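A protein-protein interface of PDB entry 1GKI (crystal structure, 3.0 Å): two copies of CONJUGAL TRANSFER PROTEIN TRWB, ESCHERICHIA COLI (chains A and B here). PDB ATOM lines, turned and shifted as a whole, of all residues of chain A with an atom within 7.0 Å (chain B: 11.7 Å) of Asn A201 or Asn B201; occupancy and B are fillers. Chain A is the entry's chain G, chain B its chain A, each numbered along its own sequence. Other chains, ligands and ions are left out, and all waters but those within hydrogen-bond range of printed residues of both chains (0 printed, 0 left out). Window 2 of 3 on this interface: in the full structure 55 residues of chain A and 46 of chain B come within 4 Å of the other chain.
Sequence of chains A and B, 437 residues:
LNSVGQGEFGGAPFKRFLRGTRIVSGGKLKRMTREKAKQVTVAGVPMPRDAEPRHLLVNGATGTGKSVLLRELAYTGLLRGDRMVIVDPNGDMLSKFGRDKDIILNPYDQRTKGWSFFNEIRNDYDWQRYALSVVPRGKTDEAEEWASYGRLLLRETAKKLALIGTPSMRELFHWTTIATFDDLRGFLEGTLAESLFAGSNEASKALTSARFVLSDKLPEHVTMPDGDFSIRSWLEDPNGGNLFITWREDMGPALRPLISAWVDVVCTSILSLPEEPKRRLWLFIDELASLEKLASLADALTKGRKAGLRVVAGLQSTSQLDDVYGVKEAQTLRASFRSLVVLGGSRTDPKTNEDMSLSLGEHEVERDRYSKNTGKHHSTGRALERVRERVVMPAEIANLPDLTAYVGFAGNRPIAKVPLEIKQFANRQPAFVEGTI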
ATOM      1  N   PHE A 181     -24.349  13.926 -25.349  1.00  0.00           N
ATOM      2  CA  PHE A 181     -23.392  14.943 -25.754  1.00  0.00           C
ATOM      3  C   PHE A 181     -24.040  16.075 -26.541  1.00  0.00           C
ATOM      4  O   PHE A 181     -23.866  17.254 -26.220  1.00  0.00           O
ATOM      5  CB  PHE A 181     -22.287  14.293 -26.595  1.00  0.00           C
ATOM      6  CG  PHE A 181     -20.898  14.632 -26.136  1.00  0.00           C
ATOM      7  CD1 PHE A 181     -20.493  14.354 -24.826  1.00  0.00           C
ATOM      8  CD2 PHE A 181     -19.995  15.232 -27.009  1.00  0.00           C
ATOM      9  CE1 PHE A 181     -19.209  14.669 -24.390  1.00  0.00           C
ATOM     10  CE2 PHE A 181     -18.705  15.553 -26.589  1.00  0.00           C
ATOM     11  CZ  PHE A 181     -18.308  15.271 -25.274  1.00  0.00           C
ATOM     12  N   ALA A 198     -16.796  22.902 -28.577  1.00  0.00           N
ATOM     13  CA  ALA A 198     -17.147  22.389 -29.900  1.00  0.00           C
ATOM     14  C   ALA A 198     -16.240  22.942 -30.995  1.00  0.00           C
ATOM     15  O   ALA A 198     -15.627  24.001 -30.830  1.00  0.00           O
ATOM     16  CB  ALA A 198     -18.602  22.712 -30.212  1.00  0.00           C
ATOM     17  N   GLY A 199     -16.146  22.210 -32.105  1.00  0.00           N
ATOM     18  CA  GLY A 199     -15.330  22.655 -33.222  1.00  0.00           C
ATOM     19  C   GLY A 199     -14.064  21.874 -33.510  1.00  0.00           C
ATOM     20  O   GLY A 199     -13.413  22.108 -34.529  1.00  0.00           O
ATOM     21  N   SER A 200     -13.701  20.952 -32.627  1.00  0.00           N
ATOM     22  CA  SER A 200     -12.493  20.158 -32.822  1.00  0.00           C
ATOM     23  C   SER A 200     -12.546  18.949 -31.912  1.00  0.00           C
ATOM     24  O   SER A 200     -13.405  18.862 -31.037  1.00  0.00           O
ATOM     25  CB  SER A 200     -11.239  20.972 -32.477  1.00  0.00           C
ATOM     26  OG  SER A 200     -11.123  21.171 -31.075  1.00  0.00           O
ATOM     27  N   ASN A 201     -11.633  18.010 -32.113  1.00  0.00           N
ATOM     28  CA  ASN A 201     -11.615  16.846 -31.252  1.00  0.00           C
ATOM     29  C   ASN A 201     -11.224  17.324 -29.869  1.00  0.00           C
ATOM     30  O   ASN A 201     -11.800  16.896 -28.876  1.00  0.00           O
ATOM     31  CB  ASN A 201     -10.601  15.814 -31.739  1.00  0.00           C
ATOM     32  CG  ASN A 201     -11.025  15.146 -33.030  1.00  0.00           C
ATOM     33  OD1 ASN A 201     -12.111  14.568 -33.119  1.00  0.00           O
ATOM     34  ND2 ASN A 201     -10.164  15.211 -34.041  1.00  0.00           N
ATOM     35  N   GLU A 202     -10.249  18.228 -29.812  1.00  0.00           N
ATOM     36  CA  GLU A 202      -9.769  18.746 -28.541  1.00  0.00           C
ATOM     37  C   GLU A 202     -10.932  19.274 -27.741  1.00  0.00           C
ATOM     38  O   GLU A 202     -11.076  18.952 -26.561  1.00  0.00           O
ATOM     39  CB  GLU A 202      -8.745  19.857 -28.760  1.00  0.00           C
ATOM     40  CG  GLU A 202      -8.079  20.321 -27.475  1.00  0.00           C
ATOM     41  CD  GLU A 202      -7.365  19.192 -26.746  1.00  0.00           C
ATOM     42  OE1 GLU A 202      -6.975  19.382 -25.572  1.00  0.00           O
ATOM     43  OE2 GLU A 202      -7.183  18.113 -27.347  1.00  0.00           O
ATOM     44  N   ALA A 203     -11.760  20.086 -28.393  1.00  0.00           N
ATOM     45  CA  ALA A 203     -12.935  20.665 -27.755  1.00  0.00           C
ATOM     46  C   ALA A 203     -13.803  19.566 -27.153  1.00  0.00           C
ATOM     47  O   ALA A 203     -14.205  19.647 -25.992  1.00  0.00           O
ATOM     48  CB  ALA A 203     -13.736  21.459 -28.772  1.00  0.00           C
ATOM     49  N   SER A 204     -14.085  18.542 -27.954  1.00  0.00           N
ATOM     50  CA  SER A 204     -14.898  17.411 -27.523  1.00  0.00           C
ATOM     51  C   SER A 204     -14.239  16.655 -26.386  1.00  0.00           C
ATOM     52  O   SER A 204     -14.908  16.225 -25.457  1.00  0.00           O
ATOM     53  CB  SER A 204     -15.136  16.457 -28.689  1.00  0.00           C
ATOM     54  OG  SER A 204     -15.957  17.060 -29.672  1.00  0.00           O
ATOM     55  N   LYS A 205     -12.928  16.481 -26.471  1.00  0.00           N
ATOM     56  CA  LYS A 205     -12.189  15.795 -25.432  1.00  0.00           C
ATOM     57  C   LYS A 205     -12.357  16.579 -24.124  1.00  0.00           C
ATOM     58  O   LYS A 205     -12.639  16.010 -23.074  1.00  0.00           O
ATOM     59  CB  LYS A 205     -10.710  15.717 -25.816  1.00  0.00           C
ATOM     60  CG  LYS A 205      -9.851  15.015 -24.782  1.00  0.00           C
ATOM     61  CD  LYS A 205      -8.378  15.235 -25.040  1.00  0.00           C
ATOM     62  CE  LYS A 205      -7.536  14.804 -23.842  1.00  0.00           C
ATOM     63  NZ  LYS A 205      -6.137  15.323 -23.940  1.00  0.00           N
ATOM     64  N   ALA A 206     -12.192  17.894 -24.202  1.00  0.00           N
ATOM     65  CA  ALA A 206     -12.327  18.756 -23.034  1.00  0.00           C
ATOM     66  C   ALA A 206     -13.695  18.577 -22.388  1.00  0.00           C
ATOM     67  O   ALA A 206     -13.800  18.468 -21.167  1.00  0.00           O
ATOM     68  CB  ALA A 206     -12.118  20.218 -23.432  1.00  0.00           C
ATOM     69  N   LEU A 207     -14.745  18.554 -23.205  1.00  0.00           N
ATOM     70  CA  LEU A 207     -16.095  18.380 -22.689  1.00  0.00           C
ATOM     71  C   LEU A 207     -16.187  17.032 -21.983  1.00  0.00           C
ATOM     72  O   LEU A 207     -16.752  16.933 -20.903  1.00  0.00           O
ATOM     73  CB  LEU A 207     -17.112  18.421 -23.827  1.00  0.00           C
ATOM     74  CG  LEU A 207     -18.489  19.057 -23.591  1.00  0.00           C
ATOM     75  CD1 LEU A 207     -19.500  18.290 -24.431  1.00  0.00           C
ATOM     76  CD2 LEU A 207     -18.891  19.026 -22.124  1.00  0.00           C
ATOM     77  N   THR A 208     -15.629  15.994 -22.593  1.00  0.00           N
ATOM     78  CA  THR A 208     -15.655  14.665 -21.995  1.00  0.00           C
ATOM     79  C   THR A 208     -14.959  14.693 -20.647  1.00  0.00           C
ATOM     80  O   THR A 208     -15.404  14.051 -19.699  1.00  0.00           O
ATOM     81  CB  THR A 208     -14.971  13.614 -22.896  1.00  0.00           C
ATOM     82  OG1 THR A 208     -15.745  13.425 -24.085  1.00  0.00           O
ATOM     83  CG2 THR A 208     -14.860  12.288 -22.182  1.00  0.00           C
ATOM     84  N   GLU B 145      -5.978   6.591 -13.362  1.00  0.00           N
ATOM     85  CA  GLU B 145      -7.043   7.199 -14.126  1.00  0.00           C
ATOM     86  C   GLU B 145      -7.807   6.078 -14.834  1.00  0.00           C
ATOM     87  O   GLU B 145      -9.040   6.060 -14.848  1.00  0.00           O
ATOM     88  CB  GLU B 145      -6.470   8.178 -15.140  1.00  0.00           C
ATOM     89  CG  GLU B 145      -7.534   8.827 -15.979  1.00  0.00           C
ATOM     90  CD  GLU B 145      -6.958   9.506 -17.176  1.00  0.00           C
ATOM     91  OE1 GLU B 145      -7.710   9.770 -18.128  1.00  0.00           O
ATOM     92  OE2 GLU B 145      -5.745   9.781 -17.166  1.00  0.00           O
ATOM     93  N   TRP B 146      -7.074   5.134 -15.419  1.00  0.00           N
ATOM     94  CA  TRP B 146      -7.718   4.019 -16.100  1.00  0.00           C
ATOM     95  C   TRP B 146      -8.524   3.250 -15.071  1.00  0.00           C
ATOM     96  O   TRP B 146      -9.686   2.920 -15.293  1.00  0.00           O
ATOM     97  CB  TRP B 146      -6.693   3.073 -16.727  1.00  0.00           C
ATOM     98  CG  TRP B 146      -5.807   3.700 -17.751  1.00  0.00           C
ATOM     99  CD1 TRP B 146      -6.137   4.703 -18.619  1.00  0.00           C
ATOM    100  CD2 TRP B 146      -4.444   3.356 -18.041  1.00  0.00           C
ATOM    101  NE1 TRP B 146      -5.064   5.009 -19.428  1.00  0.00           N
ATOM    102  CE2 TRP B 146      -4.010   4.196 -19.095  1.00  0.00           C
ATOM    103  CE3 TRP B 146      -3.542   2.416 -17.509  1.00  0.00           C
ATOM    104  CZ2 TRP B 146      -2.719   4.132 -19.631  1.00  0.00           C
ATOM    105  CZ3 TRP B 146      -2.252   2.352 -18.043  1.00  0.00           C
ATOM    106  CH2 TRP B 146      -1.856   3.207 -19.095  1.00  0.00           C
ATOM    107  N   TYR B 149     -11.819   4.616 -14.363  1.00  0.00           N
ATOM    108  CA  TYR B 149     -12.763   4.346 -15.451  1.00  0.00           C
ATOM    109  C   TYR B 149     -13.272   2.928 -15.267  1.00  0.00           C
ATOM    110  O   TYR B 149     -14.456   2.643 -15.460  1.00  0.00           O
ATOM    111  CB  TYR B 149     -12.082   4.462 -16.827  1.00  0.00           C
ATOM    112  CG  TYR B 149     -11.739   5.878 -17.238  1.00  0.00           C
ATOM    113  CD1 TYR B 149     -10.589   6.154 -17.980  1.00  0.00           C
ATOM    114  CD2 TYR B 149     -12.536   6.953 -16.839  1.00  0.00           C
ATOM    115  CE1 TYR B 149     -10.236   7.467 -18.305  1.00  0.00           C
ATOM    116  CE2 TYR B 149     -12.194   8.267 -17.158  1.00  0.00           C
ATOM    117  CZ  TYR B 149     -11.042   8.518 -17.887  1.00  0.00           C
ATOM    118  OH  TYR B 149     -10.688   9.820 -18.167  1.00  0.00           O
ATOM    119  N   PHE B 181     -18.425  -3.601 -27.997  1.00  0.00           N
ATOM    120  CA  PHE B 181     -18.507  -2.223 -27.552  1.00  0.00           C
ATOM    121  C   PHE B 181     -19.921  -1.680 -27.562  1.00  0.00           C
ATOM    122  O   PHE B 181     -20.384  -1.117 -26.567  1.00  0.00           O
ATOM    123  CB  PHE B 181     -17.634  -1.353 -28.439  1.00  0.00           C
ATOM    124  CG  PHE B 181     -16.700  -0.469 -27.676  1.00  0.00           C
ATOM    125  CD1 PHE B 181     -15.771  -1.021 -26.795  1.00  0.00           C
ATOM    126  CD2 PHE B 181     -16.752   0.913 -27.829  1.00  0.00           C
ATOM    127  CE1 PHE B 181     -14.911  -0.210 -26.081  1.00  0.00           C
ATOM    128  CE2 PHE B 181     -15.896   1.734 -27.119  1.00  0.00           C
ATOM    129  CZ  PHE B 181     -14.973   1.173 -26.242  1.00  0.00           C
ATOM    130  N   ARG B 185     -22.486  -0.611 -24.432  1.00  0.00           N
ATOM    131  CA  ARG B 185     -23.059   0.724 -24.353  1.00  0.00           C
ATOM    132  C   ARG B 185     -24.557   0.581 -24.170  1.00  0.00           C
ATOM    133  O   ARG B 185     -25.177   1.292 -23.370  1.00  0.00           O
ATOM    134  CB  ARG B 185     -22.771   1.488 -25.636  1.00  0.00           C
ATOM    135  CG  ARG B 185     -21.346   1.991 -25.753  1.00  0.00           C
ATOM    136  CD  ARG B 185     -21.364   3.499 -25.889  1.00  0.00           C
ATOM    137  NE  ARG B 185     -20.076   4.054 -26.278  1.00  0.00           N
ATOM    138  CZ  ARG B 185     -19.374   3.651 -27.333  1.00  0.00           C
ATOM    139  NH1 ARG B 185     -18.212   4.231 -27.609  1.00  0.00           N
ATOM    140  NH2 ARG B 185     -19.825   2.660 -28.099  1.00  0.00           N
ATOM    141  N   SER B 195     -24.187   7.970 -20.654  1.00  0.00           N
ATOM    142  CA  SER B 195     -23.552   8.966 -21.503  1.00  0.00           C
ATOM    143  C   SER B 195     -22.065   9.173 -21.251  1.00  0.00           C
ATOM    144  O   SER B 195     -21.324   9.536 -22.165  1.00  0.00           O
ATOM    145  CB  SER B 195     -24.284  10.308 -21.384  1.00  0.00           C
ATOM    146  OG  SER B 195     -25.551  10.244 -22.019  1.00  0.00           O
ATOM    147  N   LEU B 196     -21.617   8.943 -20.022  1.00  0.00           N
ATOM    148  CA  LEU B 196     -20.204   9.137 -19.704  1.00  0.00           C
ATOM    149  C   LEU B 196     -19.241   8.452 -20.674  1.00  0.00           C
ATOM    150  O   LEU B 196     -18.204   9.019 -21.017  1.00  0.00           O
ATOM    151  CB  LEU B 196     -19.924   8.670 -18.280  1.00  0.00           C
ATOM    152  CG  LEU B 196     -20.558   9.557 -17.209  1.00  0.00           C
ATOM    153  CD1 LEU B 196     -20.318   8.985 -15.824  1.00  0.00           C
ATOM    154  CD2 LEU B 196     -19.965  10.940 -17.313  1.00  0.00           C
ATOM    155  N   PHE B 197     -19.588   7.244 -21.120  1.00  0.00           N
ATOM    156  CA  PHE B 197     -18.745   6.478 -22.042  1.00  0.00           C
ATOM    157  C   PHE B 197     -19.136   6.616 -23.510  1.00  0.00           C
ATOM    158  O   PHE B 197     -18.979   5.675 -24.284  1.00  0.00           O
ATOM    159  CB  PHE B 197     -18.756   4.988 -21.669  1.00  0.00           C
ATOM    160  CG  PHE B 197     -17.932   4.659 -20.456  1.00  0.00           C
ATOM    161  CD1 PHE B 197     -18.451   3.861 -19.439  1.00  0.00           C
ATOM    162  CD2 PHE B 197     -16.636   5.150 -20.321  1.00  0.00           C
ATOM    163  CE1 PHE B 197     -17.689   3.560 -18.300  1.00  0.00           C
ATOM    164  CE2 PHE B 197     -15.867   4.855 -19.191  1.00  0.00           C
ATOM    165  CZ  PHE B 197     -16.399   4.059 -18.180  1.00  0.00           C
ATOM    166  N   ALA B 198     -19.639   7.784 -23.900  1.00  0.00           N
ATOM    167  CA  ALA B 198     -20.028   7.998 -25.291  1.00  0.00           C
ATOM    168  C   ALA B 198     -20.096   9.477 -25.652  1.00  0.00           C
ATOM    169  O   ALA B 198     -20.222  10.334 -24.779  1.00  0.00           O
ATOM    170  CB  ALA B 198     -21.366   7.338 -25.563  1.00  0.00           C
ATOM    171  N   GLY B 199     -19.997   9.773 -26.945  1.00  0.00           N
ATOM    172  CA  GLY B 199     -20.062  11.157 -27.390  1.00  0.00           C
ATOM    173  C   GLY B 199     -18.767  11.784 -27.890  1.00  0.00           C
ATOM    174  O   GLY B 199     -18.767  12.918 -28.372  1.00  0.00           O
ATOM    175  N   SER B 200     -17.656  11.069 -27.779  1.00  0.00           N
ATOM    176  CA  SER B 200     -16.384  11.611 -28.241  1.00  0.00           C
ATOM    177  C   SER B 200     -15.360  10.490 -28.270  1.00  0.00           C
ATOM    178  O   SER B 200     -15.607   9.405 -27.737  1.00  0.00           O
ATOM    179  CB  SER B 200     -15.894  12.714 -27.294  1.00  0.00           C
ATOM    180  OG  SER B 200     -15.413  12.155 -26.083  1.00  0.00           O
ATOM    181  N   ASN B 201     -14.217  10.743 -28.898  1.00  0.00           N
ATOM    182  CA  ASN B 201     -13.173   9.732 -28.951  1.00  0.00           C
ATOM    183  C   ASN B 201     -12.708   9.480 -27.534  1.00  0.00           C
ATOM    184  O   ASN B 201     -12.544   8.331 -27.124  1.00  0.00           O
ATOM    185  CB  ASN B 201     -11.993  10.205 -29.795  1.00  0.00           C
ATOM    186  CG  ASN B 201     -12.314  10.234 -31.268  1.00  0.00           C
ATOM    187  OD1 ASN B 201     -12.747   9.227 -31.839  1.00  0.00           O
ATOM    188  ND2 ASN B 201     -12.105  11.384 -31.898  1.00  0.00           N
ATOM    189  N   GLU B 202     -12.504  10.567 -26.790  1.00  0.00           N
ATOM    190  CA  GLU B 202     -12.056  10.476 -25.409  1.00  0.00           C
ATOM    191  C   GLU B 202     -12.967   9.528 -24.632  1.00  0.00           C
ATOM    192  O   GLU B 202     -12.495   8.628 -23.942  1.00  0.00           O
ATOM    193  CB  GLU B 202     -12.067  11.858 -24.758  1.00  0.00           C
ATOM    194  CG  GLU B 202     -11.460  11.868 -23.365  1.00  0.00           C
ATOM    195  CD  GLU B 202     -10.006  11.435 -23.372  1.00  0.00           C
ATOM    196  OE1 GLU B 202      -9.450  11.178 -22.283  1.00  0.00           O
ATOM    197  OE2 GLU B 202      -9.416  11.357 -24.470  1.00  0.00           O
ATOM    198  N   ALA B 203     -14.275   9.727 -24.753  1.00  0.00           N
ATOM    199  CA  ALA B 203     -15.232   8.875 -24.066  1.00  0.00           C
ATOM    200  C   ALA B 203     -14.961   7.407 -24.412  1.00  0.00           C
ATOM    201  O   ALA B 203     -14.868   6.552 -23.532  1.00  0.00           O
ATOM    202  CB  ALA B 203     -16.652   9.263 -24.470  1.00  0.00           C
ATOM    203  N   SER B 204     -14.829   7.123 -25.705  1.00  0.00           N
ATOM    204  CA  SER B 204     -14.568   5.764 -26.168  1.00  0.00           C
ATOM    205  C   SER B 204     -13.244   5.234 -25.642  1.00  0.00           C
ATOM    206  O   SER B 204     -13.141   4.069 -25.262  1.00  0.00           O
ATOM    207  CB  SER B 204     -14.558   5.718 -27.694  1.00  0.00           C
ATOM    208  OG  SER B 204     -15.853   5.959 -28.201  1.00  0.00           O
ATOM    209  N   LYS B 205     -12.229   6.087 -25.634  1.00  0.00           N
ATOM    210  CA  LYS B 205     -10.927   5.688 -25.143  1.00  0.00           C
ATOM    211  C   LYS B 205     -11.071   5.283 -23.687  1.00  0.00           C
ATOM    212  O   LYS B 205     -10.550   4.252 -23.268  1.00  0.00           O
ATOM    213  CB  LYS B 205      -9.945   6.848 -25.260  1.00  0.00           C
ATOM    214  CG  LYS B 205      -8.558   6.541 -24.718  1.00  0.00           C
ATOM    215  CD  LYS B 205      -7.736   7.802 -24.600  1.00  0.00           C
ATOM    216  CE  LYS B 205      -6.457   7.569 -23.810  1.00  0.00           C
ATOM    217  NZ  LYS B 205      -5.815   8.867 -23.419  1.00  0.00           N
ATOM    218  N   ALA B 206     -11.790   6.101 -22.919  1.00  0.00           N
ATOM    219  CA  ALA B 206     -12.006   5.840 -21.500  1.00  0.00           C
ATOM    220  C   ALA B 206     -12.660   4.480 -21.302  1.00  0.00           C
ATOM    221  O   ALA B 206     -12.270   3.717 -20.421  1.00  0.00           O
ATOM    222  CB  ALA B 206     -12.873   6.929 -20.892  1.00  0.00           C
ATOM    223  N   LEU B 207     -13.659   4.180 -22.123  1.00  0.00           N
ATOM    224  CA  LEU B 207     -14.343   2.904 -22.024  1.00  0.00           C
ATOM    225  C   LEU B 207     -13.352   1.787 -22.312  1.00  0.00           C
ATOM    226  O   LEU B 207     -13.349   0.771 -21.626  1.00  0.00           O
ATOM    227  CB  LEU B 207     -15.493   2.819 -23.027  1.00  0.00           C
ATOM    228  CG  LEU B 207     -16.753   2.017 -22.659  1.00  0.00           C
ATOM    229  CD1 LEU B 207     -17.347   1.458 -23.941  1.00  0.00           C
ATOM    230  CD2 LEU B 207     -16.446   0.886 -21.696  1.00  0.00           C
ATOM    231  N   THR B 208     -12.515   1.966 -23.330  1.00  0.00           N
ATOM    232  CA  THR B 208     -11.528   0.948 -23.676  1.00  0.00           C
ATOM    233  C   THR B 208     -10.568   0.738 -22.517  1.00  0.00           C
ATOM    234  O   THR B 208     -10.157  -0.387 -22.247  1.00  0.00           O
ATOM    235  CB  THR B 208     -10.723   1.327 -24.926  1.00  0.00           C
ATOM    236  OG1 THR B 208     -11.598   1.391 -26.052  1.00  0.00           O
ATOM    237  CG2 THR B 208      -9.651   0.290 -25.202  1.00  0.00           C
ATOM    238  N   SER B 209     -10.206   1.818 -21.831  1.00  0.00           N
ATOM    239  CA  SER B 209      -9.315   1.700 -20.688  1.00  0.00           C
ATOM    240  C   SER B 209     -10.000   0.856 -19.615  1.00  0.00           C
ATOM    241  O   SER B 209      -9.408  -0.082 -19.083  1.00  0.00           O
ATOM    242  CB  SER B 209      -8.989   3.077 -20.125  1.00  0.00           C
ATOM    243  OG  SER B 209      -8.285   3.839 -21.078  1.00  0.00           O
ATOM    244  N   ALA B 210     -11.252   1.186 -19.306  1.00  0.00           N
ATOM    245  CA  ALA B 210     -12.011   0.455 -18.299  1.00  0.00           C
ATOM    246  C   ALA B 210     -12.023  -1.037 -18.600  1.00  0.00           C
ATOM    247  O   ALA B 210     -11.758  -1.847 -17.720  1.00  0.00           O
ATOM    248  CB  ALA B 210     -13.429   0.982 -18.228  1.00  0.00           C
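OD1 of Asn A201 sits at hydrogen-bond distance from ND2 of Asn B201 (3.4 Å).
OG1 of Thr A208 sits close to OG of Ser B200, 2.4 Å away.
The backbone carbonyl oxygen (O) of Ser B200 is in hydrogen-bond range of the side-chain hydroxyl (OG) of Ser B204, at 3.5 Å.
N of Ala B203 is in hydrogen-bond range of OG of Ser B200 (3.0 Å).
The side-chain hydroxyl (OG) of Ser B200 sits close to the backbone NH (N) of Glu B202, at 3.4 Å.
The side-chain hydroxyl of Thr A208 lies within hydrogen-bond range of the backbone carbonyl oxygen of Ser A204 (3.2 Å).
Among the printed residues, merely in contact across the chains: Phe A181 with Gly B199, Thr A208 with Glu B202, Thr A208 with Ala B203 and Lys A205 with Glu B202.
Ala A198 touches none of the printed residues of chain B.
No residue of chain B comes within 4 Å of Gly A199.
Asn A201 touches just one residue of chain B: Asn B201.
No residue of chain B comes within 4 Å of Glu A202.
No residue of chain B comes within 4 Å of Ser A204.
Of the printed residues of chain B, Lys A205 touches Glu B202.
Of the printed residues of chain A, Gly B199 touches Phe A181 (3.0 Å).
Of chain A, only Asn A201 (3.4 Å) comes within 4 Å of Asn B201.
Of the printed residues of chain A, Ala B203 touches Thr A208.
Ser B209 touches none of the printed residues of chain A.
Of the 21 printed residues of chain B, 5 touch a printed residue of chain A.
Hydrophobic or aromatic side chains of chain A within 4 Å of the printed part of chain B: Phe A181.
Among the printed residues, 6 pairs touch across the chains.
Among the printed residues, no Asp or Glu carboxylate lies within 4 Å of a Lys or Arg side-chain nitrogen of the other chain.
Asn A201 touches its own counterpart, Asn B201.
Lys A205 touches Glu B202, but with the chains exchanged Glu A202 does not touch Lys B205 (10.1 Å).
Thr A208 touches Ser B200, but with the chains exchanged Ser A200 does not touch Thr B208 (18.3 Å).
Thr A208 touches Ala B203, but with the chains exchanged Ala A203 does not touch Thr B208 (18.0 Å).
Positions printed for both chains: 181, 198, 199, 200, 201, 202, 203, 204, 205, 206, 207 and 208.
Of the 6 pairs that touch across the chains among the printed residues, 1 has its exchanged pair printed and touching as well.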
